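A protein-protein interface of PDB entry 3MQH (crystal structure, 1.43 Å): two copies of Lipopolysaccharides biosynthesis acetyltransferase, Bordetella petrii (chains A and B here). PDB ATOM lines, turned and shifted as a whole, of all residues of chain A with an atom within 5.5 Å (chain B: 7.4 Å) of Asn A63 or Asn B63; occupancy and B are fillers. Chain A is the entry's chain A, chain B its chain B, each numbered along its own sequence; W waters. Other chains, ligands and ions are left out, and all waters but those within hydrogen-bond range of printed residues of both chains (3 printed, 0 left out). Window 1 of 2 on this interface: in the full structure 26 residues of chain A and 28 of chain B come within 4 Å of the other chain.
The side-chain amide nitrogen (ND2) of Asn B62 is in hydrogen-bond range of the side-chain hydroxyl (OG) of Ser A65 (3.0 Å). NE2 of Gln B44 lies within hydrogen-bond range of OD1 of Asn A45, 3.0 Å away. ND2 of Asn A45 sits at hydrogen-bond distance from OD1 of Asn B63, 2.8 Å away. The side-chain amide nitrogen (NE2) of Gln B44 is in hydrogen-bond range of the backbone carbonyl oxygen (O) of Val A46 (3.3 Å).
O of Gln A44 is in hydrogen-bond range of N of Asn A63 (3.0 Å). ND2 of Asn A45 lies within hydrogen-bond range of OD1 of Asn A63, 2.9 Å away. The backbone carbonyl oxygen (O) of Gln B44 lies within hydrogen-bond range of the backbone NH (N) of Asn B63 (3.0 Å). The backbone NH of Gln B44 lies within hydrogen-bond range of the side-chain amide oxygen of Asn B62 (2.9 Å). N of Ser B81 is in hydrogen-bond range of O of Asn B62 (2.9 Å). The side-chain amide nitrogen (ND2) of Asn B45 sits at hydrogen-bond distance from the side-chain amide oxygen (OD1) of Asn B63, 2.9 Å away.
Among the printed residues, pairs that only touch across the chains: Asn A45 with Asn B45, Ser A65 with Asn B63 and Asn A63 with Asn B63.
Asn A63 touches just one residue of chain B: Asn B63. Of the printed residues of chain B, Ser A65 touches Asn B62 and Asn B63. Of the printed residues of chain A, Gln B44 touches Asn A45 and Val A46. Of the printed residues of chain A, Asn B45 touches Asn A45 (3.4 Å). Of the printed residues of chain B, Val A46 touches Gln B44. Printed residues of chain A within 4 Å of Asn B62: Ser A65 (3.0 Å). Ser B65 touches none of the printed residues of chain A. Phe B47 touches none of the printed residues of chain A. The nearest printed residue of chain A that does not touch Asn B45 is Asn A63 (5.2 Å).
Of the 18 printed residues of chain B, 4 touch a printed residue of chain A. Of the 11 printed residues of chain A, 4 touch a printed residue of chain B.
Asn A45 touches Gln B44, but with the chains exchanged Gln A44 does not touch Asn B45 (7.5 Å). Asn A45 touches Asn B63, but with the chains exchanged Asn A63 does not touch Asn B45 (5.2 Å). Val A46 touches Gln B44, but with the chains exchanged Gln A44 does not touch Val B46 (11.9 Å). Ser A65 touches Asn B62, but with the chains exchanged Asn A62 does not touch Ser B65 (13.6 Å).
Water W1 lies within hydrogen-bond range of the side-chain hydroxyl (OG) of Ser B81 (2.7 Å) and the backbone carbonyl oxygen (O) of Asn A63 (2.7 Å). Water W2 lies within hydrogen-bond range of the backbone carbonyl oxygen of Asn A45, the side-chain amide nitrogen of Asn B63 and the side-chain hydroxyl of Ser A65. Water W3 lies within hydrogen-bond range of OG of Ser B81 (2.7 Å), OG of Ser A65 (2.8 Å) and ND2 of Asn B63 (3.1 Å).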
ATOM      1  N   GLY A  43     -23.436 -24.308  -5.674  1.00  0.00           N
ATOM      2  CA  GLY A  43     -24.210 -25.360  -5.024  1.00  0.00           C
ATOM      3  C   GLY A  43     -25.385 -24.926  -4.160  1.00  0.00           C
ATOM      4  O   GLY A  43     -25.721 -23.733  -4.058  1.00  0.00           O
ATOM      5  N   GLN A  44     -25.970 -25.916  -3.484  1.00  0.00           N
ATOM      6  CA  GLN A  44     -27.192 -25.717  -2.703  1.00  0.00           C
ATOM      7  C   GLN A  44     -27.026 -24.545  -1.741  1.00  0.00           C
ATOM      8  O   GLN A  44     -25.995 -24.490  -1.047  1.00  0.00           O
ATOM      9  CB  GLN A  44     -27.533 -27.004  -1.961  1.00  0.00           C
ATOM     10  CG  GLN A  44     -28.737 -26.950  -1.073  1.00  0.00           C
ATOM     11  CD  GLN A  44     -29.131 -28.309  -0.590  1.00  0.00           C
ATOM     12  OE1 GLN A  44     -29.227 -29.276  -1.345  1.00  0.00           O
ATOM     13  NE2 GLN A  44     -29.368 -28.422   0.710  1.00  0.00           N
ATOM     14  N   ASN A  45     -27.971 -23.623  -1.651  1.00  0.00           N
ATOM     15  CA  ASN A  45     -28.016 -22.591  -0.626  1.00  0.00           C
ATOM     16  C   ASN A  45     -26.902 -21.544  -0.737  1.00  0.00           C
ATOM     17  O   ASN A  45     -26.701 -20.748   0.210  1.00  0.00           O
ATOM     18  CB  ASN A  45     -28.097 -23.205   0.780  1.00  0.00           C
ATOM     19  CG  ASN A  45     -28.185 -22.168   1.895  1.00  0.00           C
ATOM     20  OD1 ASN A  45     -29.096 -21.304   1.900  1.00  0.00           O
ATOM     21  ND2 ASN A  45     -27.266 -22.233   2.895  1.00  0.00           N
ATOM     22  N   VAL A  46     -26.222 -21.487  -1.887  1.00  0.00           N
ATOM     23  CA  VAL A  46     -25.296 -20.365  -2.066  1.00  0.00           C
ATOM     24  C   VAL A  46     -26.069 -19.058  -2.035  1.00  0.00           C
ATOM     25  O   VAL A  46     -27.269 -18.986  -2.457  1.00  0.00           O
ATOM     26  CB  VAL A  46     -24.464 -20.597  -3.324  1.00  0.00           C
ATOM     27  CG1 VAL A  46     -23.843 -19.339  -3.882  1.00  0.00           C
ATOM     28  CG2 VAL A  46     -23.389 -21.700  -3.006  1.00  0.00           C
ATOM     29  N   GLN A  61     -19.056 -24.604  -3.725  1.00  0.00           N
ATOM     30  CA  GLN A  61     -19.785 -25.696  -3.097  1.00  0.00           C
ATOM     31  C   GLN A  61     -20.927 -25.188  -2.212  1.00  0.00           C
ATOM     32  O   GLN A  61     -21.093 -23.976  -2.004  1.00  0.00           O
ATOM     33  CB  GLN A  61     -18.818 -26.619  -2.346  1.00  0.00           C
ATOM     34  CG  GLN A  61     -17.661 -27.180  -3.204  1.00  0.00           C
ATOM     35  CD  GLN A  61     -18.120 -27.768  -4.543  1.00  0.00           C
ATOM     36  OE1 GLN A  61     -19.057 -28.574  -4.619  1.00  0.00           O
ATOM     37  NE2 GLN A  61     -17.414 -27.362  -5.603  1.00  0.00           N
ATOM     38  N   ASN A  62     -21.696 -26.139  -1.692  1.00  0.00           N
ATOM     39  CA  ASN A  62     -22.852 -25.782  -0.866  1.00  0.00           C
ATOM     40  C   ASN A  62     -22.555 -24.772   0.247  1.00  0.00           C
ATOM     41  O   ASN A  62     -21.477 -24.803   0.852  1.00  0.00           O
ATOM     42  CB  ASN A  62     -23.436 -27.024  -0.201  1.00  0.00           C
ATOM     43  CG  ASN A  62     -23.999 -28.043  -1.183  1.00  0.00           C
ATOM     44  OD1 ASN A  62     -24.018 -27.817  -2.386  1.00  0.00           O
ATOM     45  ND2 ASN A  62     -24.410 -29.184  -0.660  1.00  0.00           N
ATOM     46  N   ASN A  63     -23.499 -23.894   0.562  1.00  0.00           N
ATOM     47  CA  ASN A  63     -23.480 -23.113   1.796  1.00  0.00           C
ATOM     48  C   ASN A  63     -22.399 -22.056   1.828  1.00  0.00           C
ATOM     49  O   ASN A  63     -21.932 -21.688   2.917  1.00  0.00           O
ATOM     50  CB  ASN A  63     -23.405 -24.002   3.030  1.00  0.00           C
ATOM     51  CG  ASN A  63     -24.573 -24.967   3.079  1.00  0.00           C
ATOM     52  OD1 ASN A  63     -25.673 -24.635   2.582  1.00  0.00           O
ATOM     53  ND2 ASN A  63     -24.350 -26.158   3.583  1.00  0.00           N
ATOM     54  N   VAL A  64     -22.010 -21.557   0.661  1.00  0.00           N
ATOM     55  CA  VAL A  64     -21.077 -20.423   0.593  1.00  0.00           C
ATOM     56  C   VAL A  64     -21.847 -19.126   0.294  1.00  0.00           C
ATOM     57  O   VAL A  64     -22.625 -19.075  -0.694  1.00  0.00           O
ATOM     58  CB  VAL A  64     -19.997 -20.681  -0.494  1.00  0.00           C
ATOM     59  CG1 VAL A  64     -19.099 -19.419  -0.617  1.00  0.00           C
ATOM     60  CG2 VAL A  64     -19.186 -21.904  -0.078  1.00  0.00           C
ATOM     61  N   SER A  65     -21.667 -18.113   1.106  1.00  0.00           N
ATOM     62  CA  SER A  65     -22.237 -16.786   0.912  1.00  0.00           C
ATOM     63  C   SER A  65     -21.195 -15.820   0.362  1.00  0.00           C
ATOM     64  O   SER A  65     -20.242 -15.450   1.055  1.00  0.00           O
ATOM     65  CB  SER A  65     -22.798 -16.258   2.243  1.00  0.00           C
ATOM     66  OG  SER A  65     -23.846 -17.101   2.717  1.00  0.00           O
ATOM     67  N   SER A  81     -19.154 -24.948   2.572  1.00  0.00           N
ATOM     68  CA  SER A  81     -19.371 -24.142   3.766  1.00  0.00           C
ATOM     69  C   SER A  81     -18.203 -23.241   4.095  1.00  0.00           C
ATOM     70  O   SER A  81     -18.099 -22.858   5.250  1.00  0.00           O
ATOM     71  CB  SER A  81     -19.723 -25.052   4.927  1.00  0.00           C
ATOM     72  OG  SER A  81     -20.889 -25.797   4.606  1.00  0.00           O
ATOM     73  N   MET A  82     -17.341 -22.892   3.144  1.00  0.00           N
ATOM     74  CA  MET A  82     -16.379 -21.849   3.473  1.00  0.00           C
ATOM     75  C   MET A  82     -17.065 -20.492   3.624  1.00  0.00           C
ATOM     76  O   MET A  82     -18.202 -20.320   3.175  1.00  0.00           O
ATOM     77  CB  MET A  82     -15.132 -21.842   2.586  1.00  0.00           C
ATOM     78  CG  MET A  82     -15.308 -21.464   1.103  1.00  0.00           C
ATOM     79  SD  MET A  82     -15.660 -19.735   0.804  1.00  0.00           S
ATOM     80  CE  MET A  82     -14.316 -18.904   1.670  1.00  0.00           C
ATOM     81  N   LEU B  42     -32.776 -11.411  10.046  1.00  0.00           N
ATOM     82  CA  LEU B  42     -32.422 -12.832   9.978  1.00  0.00           C
ATOM     83  C   LEU B  42     -32.167 -13.201   8.541  1.00  0.00           C
ATOM     84  O   LEU B  42     -33.063 -13.158   7.690  1.00  0.00           O
ATOM     85  CB  LEU B  42     -33.563 -13.680  10.564  1.00  0.00           C
ATOM     86  CG  LEU B  42     -33.580 -13.871  12.094  1.00  0.00           C
ATOM     87  CD1 LEU B  42     -33.767 -12.544  12.866  1.00  0.00           C
ATOM     88  CD2 LEU B  42     -34.695 -14.863  12.523  1.00  0.00           C
ATOM     89  N   GLY B  43     -30.926 -13.577   8.220  1.00  0.00           N
ATOM     90  CA  GLY B  43     -30.514 -13.851   6.851  1.00  0.00           C
ATOM     91  C   GLY B  43     -30.962 -15.189   6.307  1.00  0.00           C
ATOM     92  O   GLY B  43     -31.676 -15.949   6.953  1.00  0.00           O
ATOM     93  N   GLN B  44     -30.522 -15.435   5.087  1.00  0.00           N
ATOM     94  CA  GLN B  44     -30.838 -16.640   4.357  1.00  0.00           C
ATOM     95  C   GLN B  44     -30.652 -17.916   5.164  1.00  0.00           C
ATOM     96  O   GLN B  44     -29.577 -18.082   5.757  1.00  0.00           O
ATOM     97  CB  GLN B  44     -30.022 -16.681   3.063  1.00  0.00           C
ATOM     98  CG  GLN B  44     -30.427 -17.861   2.155  1.00  0.00           C
ATOM     99  CD  GLN B  44     -29.770 -17.749   0.778  1.00  0.00           C
ATOM    100  OE1 GLN B  44     -29.877 -16.717   0.125  1.00  0.00           O
ATOM    101  NE2 GLN B  44     -29.050 -18.796   0.343  1.00  0.00           N
ATOM    102  N   ASN B  45     -31.633 -18.810   5.207  1.00  0.00           N
ATOM    103  CA  ASN B  45     -31.498 -20.147   5.784  1.00  0.00           C
ATOM    104  C   ASN B  45     -31.275 -20.111   7.298  1.00  0.00           C
ATOM    105  O   ASN B  45     -30.954 -21.152   7.863  1.00  0.00           O
ATOM    106  CB  ASN B  45     -30.432 -20.982   5.038  1.00  0.00           C
ATOM    107  CG  ASN B  45     -30.254 -22.379   5.612  1.00  0.00           C
ATOM    108  OD1 ASN B  45     -31.208 -23.165   5.714  1.00  0.00           O
ATOM    109  ND2 ASN B  45     -28.996 -22.696   6.008  1.00  0.00           N
ATOM    110  N   VAL B  46     -31.528 -18.998   7.986  1.00  0.00           N
ATOM    111  CA  VAL B  46     -31.509 -19.041   9.457  1.00  0.00           C
ATOM    112  C   VAL B  46     -32.597 -19.993   9.939  1.00  0.00           C
ATOM    113  O   VAL B  46     -33.653 -20.165   9.271  1.00  0.00           O
ATOM    114  CB  VAL B  46     -31.683 -17.605  10.015  1.00  0.00           C
ATOM    115  CG1 VAL B  46     -32.110 -17.571  11.452  1.00  0.00           C
ATOM    116  CG2 VAL B  46     -30.350 -16.856   9.799  1.00  0.00           C
ATOM    117  N   PHE B  47     -32.335 -20.610  11.093  1.00  0.00           N
ATOM    118  CA  PHE B  47     -33.320 -21.421  11.773  1.00  0.00           C
ATOM    119  C   PHE B  47     -33.445 -20.890  13.180  1.00  0.00           C
ATOM    120  O   PHE B  47     -32.447 -20.517  13.771  1.00  0.00           O
ATOM    121  CB  PHE B  47     -32.838 -22.909  11.846  1.00  0.00           C
ATOM    122  CG  PHE B  47     -33.661 -23.712  12.807  1.00  0.00           C
ATOM    123  CD1 PHE B  47     -34.923 -24.154  12.419  1.00  0.00           C
ATOM    124  CD2 PHE B  47     -33.227 -23.984  14.082  1.00  0.00           C
ATOM    125  CE1 PHE B  47     -35.729 -24.845  13.329  1.00  0.00           C
ATOM    126  CE2 PHE B  47     -34.008 -24.701  15.006  1.00  0.00           C
ATOM    127  CZ  PHE B  47     -35.296 -25.123  14.614  1.00  0.00           C
ATOM    128  N   ILE B  60     -28.544 -11.264  12.523  1.00  0.00           N
ATOM    129  CA  ILE B  60     -28.117 -12.647  12.350  1.00  0.00           C
ATOM    130  C   ILE B  60     -27.912 -12.872  10.867  1.00  0.00           C
ATOM    131  O   ILE B  60     -28.821 -12.775  10.039  1.00  0.00           O
ATOM    132  CB  ILE B  60     -29.190 -13.572  12.914  1.00  0.00           C
ATOM    133  CG1 ILE B  60     -29.469 -13.232  14.377  1.00  0.00           C
ATOM    134  CG2 ILE B  60     -28.801 -15.053  12.669  1.00  0.00           C
ATOM    135  CD1 ILE B  60     -30.642 -14.008  14.955  1.00  0.00           C
ATOM    136  N   GLN B  61     -26.670 -13.214  10.518  1.00  0.00           N
ATOM    137  CA  GLN B  61     -26.286 -13.399   9.141  1.00  0.00           C
ATOM    138  C   GLN B  61     -26.680 -14.800   8.662  1.00  0.00           C
ATOM    139  O   GLN B  61     -27.224 -15.612   9.404  1.00  0.00           O
ATOM    140  CB  GLN B  61     -24.788 -13.103   8.904  1.00  0.00           C
ATOM    141  CG  GLN B  61     -24.347 -11.715   9.335  1.00  0.00           C
ATOM    142  CD  GLN B  61     -25.253 -10.598   8.824  1.00  0.00           C
ATOM    143  OE1 GLN B  61     -25.576 -10.507   7.611  1.00  0.00           O
ATOM    144  NE2 GLN B  61     -25.648  -9.715   9.738  1.00  0.00           N
ATOM    145  N   ASN B  62     -26.490 -15.064   7.365  1.00  0.00           N
ATOM    146  CA  ASN B  62     -26.893 -16.341   6.755  1.00  0.00           C
ATOM    147  C   ASN B  62     -26.412 -17.553   7.540  1.00  0.00           C
ATOM    148  O   ASN B  62     -25.309 -17.557   8.115  1.00  0.00           O
ATOM    149  CB  ASN B  62     -26.297 -16.432   5.351  1.00  0.00           C
ATOM    150  CG  ASN B  62     -26.852 -15.420   4.359  1.00  0.00           C
ATOM    151  OD1 ASN B  62     -27.738 -14.627   4.655  1.00  0.00           O
ATOM    152  ND2 ASN B  62     -26.262 -15.406   3.171  1.00  0.00           N
ATOM    153  N   ASN B  63     -27.254 -18.583   7.567  1.00  0.00           N
ATOM    154  CA  ASN B  63     -26.805 -19.925   7.928  1.00  0.00           C
ATOM    155  C   ASN B  63     -26.523 -20.042   9.422  1.00  0.00           C
ATOM    156  O   ASN B  63     -25.707 -20.887   9.848  1.00  0.00           O
ATOM    157  CB  ASN B  63     -25.555 -20.397   7.127  1.00  0.00           C
ATOM    158  CG  ASN B  63     -25.897 -20.416   5.646  1.00  0.00           C
ATOM    159  OD1 ASN B  63     -27.055 -20.718   5.267  1.00  0.00           O
ATOM    160  ND2 ASN B  63     -24.941 -20.068   4.816  1.00  0.00           N
ATOM    161  N   VAL B  64     -27.191 -19.245  10.254  1.00  0.00           N
ATOM    162  CA  VAL B  64     -27.140 -19.410  11.704  1.00  0.00           C
ATOM    163  C   VAL B  64     -28.390 -20.124  12.245  1.00  0.00           C
ATOM    164  O   VAL B  64     -29.516 -19.684  11.931  1.00  0.00           O
ATOM    165  CB  VAL B  64     -26.957 -18.041  12.393  1.00  0.00           C
ATOM    166  CG1 VAL B  64     -26.937 -18.187  13.927  1.00  0.00           C
ATOM    167  CG2 VAL B  64     -25.616 -17.385  11.900  1.00  0.00           C
ATOM    168  N   SER B  65     -28.172 -21.201  12.994  1.00  0.00           N
ATOM    169  CA  SER B  65     -29.239 -21.955  13.658  1.00  0.00           C
ATOM    170  C   SER B  65     -29.304 -21.556  15.109  1.00  0.00           C
ATOM    171  O   SER B  65     -28.413 -21.882  15.868  1.00  0.00           O
ATOM    172  CB  SER B  65     -29.072 -23.469  13.465  1.00  0.00           C
ATOM    173  OG  SER B  65     -29.072 -23.797  12.089  1.00  0.00           O
ATOM    174  N   VAL B  66     -30.354 -20.853  15.533  1.00  0.00           N
ATOM    175  CA  VAL B  66     -30.464 -20.417  16.933  1.00  0.00           C
ATOM    176  C   VAL B  66     -31.331 -21.451  17.618  1.00  0.00           C
ATOM    177  O   VAL B  66     -32.554 -21.409  17.499  1.00  0.00           O
ATOM    178  CB  VAL B  66     -31.085 -18.995  17.057  1.00  0.00           C
ATOM    179  CG1 VAL B  66     -30.928 -18.495  18.488  1.00  0.00           C
ATOM    180  CG2 VAL B  66     -30.341 -17.987  16.136  1.00  0.00           C
ATOM    181  N   GLY B  79     -22.370 -13.528  13.256  1.00  0.00           N
ATOM    182  CA  GLY B  79     -21.756 -13.493  11.931  1.00  0.00           C
ATOM    183  C   GLY B  79     -22.139 -14.693  11.070  1.00  0.00           C
ATOM    184  O   GLY B  79     -22.718 -15.664  11.517  1.00  0.00           O
ATOM    185  N   PRO B  80     -21.790 -14.614   9.779  1.00  0.00           N
ATOM    186  CA  PRO B  80     -22.238 -15.634   8.824  1.00  0.00           C
ATOM    187  C   PRO B  80     -21.762 -16.984   9.302  1.00  0.00           C
ATOM    188  O   PRO B  80     -20.583 -17.166   9.607  1.00  0.00           O
ATOM    189  CB  PRO B  80     -21.547 -15.218   7.529  1.00  0.00           C
ATOM    190  CG  PRO B  80     -20.472 -14.293   7.941  1.00  0.00           C
ATOM    191  CD  PRO B  80     -20.938 -13.583   9.172  1.00  0.00           C
ATOM    192  N   SER B  81     -22.708 -17.932   9.299  1.00  0.00           N
ATOM    193  CA  SER B  81     -22.437 -19.352   9.524  1.00  0.00           C
ATOM    194  C   SER B  81     -21.822 -19.573  10.918  1.00  0.00           C
ATOM    195  O   SER B  81     -21.196 -20.625  11.148  1.00  0.00           O
ATOM    196  CB  SER B  81     -21.553 -19.891   8.381  1.00  0.00           C
ATOM    197  OG  SER B  81     -22.167 -19.705   7.112  1.00  0.00           O
ATOM    198  N   MET B  82     -22.011 -18.661  11.876  1.00  0.00           N
ATOM    199  CA  MET B  82     -21.609 -19.054  13.223  1.00  0.00           C
ATOM    200  C   MET B  82     -22.573 -20.133  13.765  1.00  0.00           C
ATOM    201  O   MET B  82     -23.687 -20.343  13.225  1.00  0.00           O
ATOM    202  CB  MET B  82     -21.393 -17.843  14.167  1.00  0.00           C
ATOM    203  CG  MET B  82     -22.622 -16.956  14.546  1.00  0.00           C
ATOM    204  SD  MET B  82     -23.738 -17.748  15.649  1.00  0.00           S
ATOM    205  CE  MET B  82     -22.712 -18.253  17.045  1.00  0.00           C
ATOM    206  N   VAL B  83     -22.124 -20.845  14.804  1.00  0.00           N
ATOM    207  CA  VAL B  83     -22.794 -22.071  15.225  1.00  0.00           C
ATOM    208  C   VAL B  83     -23.017 -22.093  16.720  1.00  0.00           C
ATOM    209  O   VAL B  83     -22.076 -22.039  17.509  1.00  0.00           O
ATOM    210  CB  VAL B  83     -22.015 -23.317  14.760  1.00  0.00           C
ATOM    211  CG1 VAL B  83     -22.722 -24.576  15.236  1.00  0.00           C
ATOM    212  CG2 VAL B  83     -21.854 -23.264  13.217  1.00  0.00           C
HETATM  213  O   HOH W   1     -21.719 -21.872   5.603  1.00  0.00           O
HETATM  214  O   HOH W   2     -24.896 -19.785   1.942  1.00  0.00           O
HETATM  215  O   HOH W   3     -22.579 -18.026   5.027  1.00  0.00           O
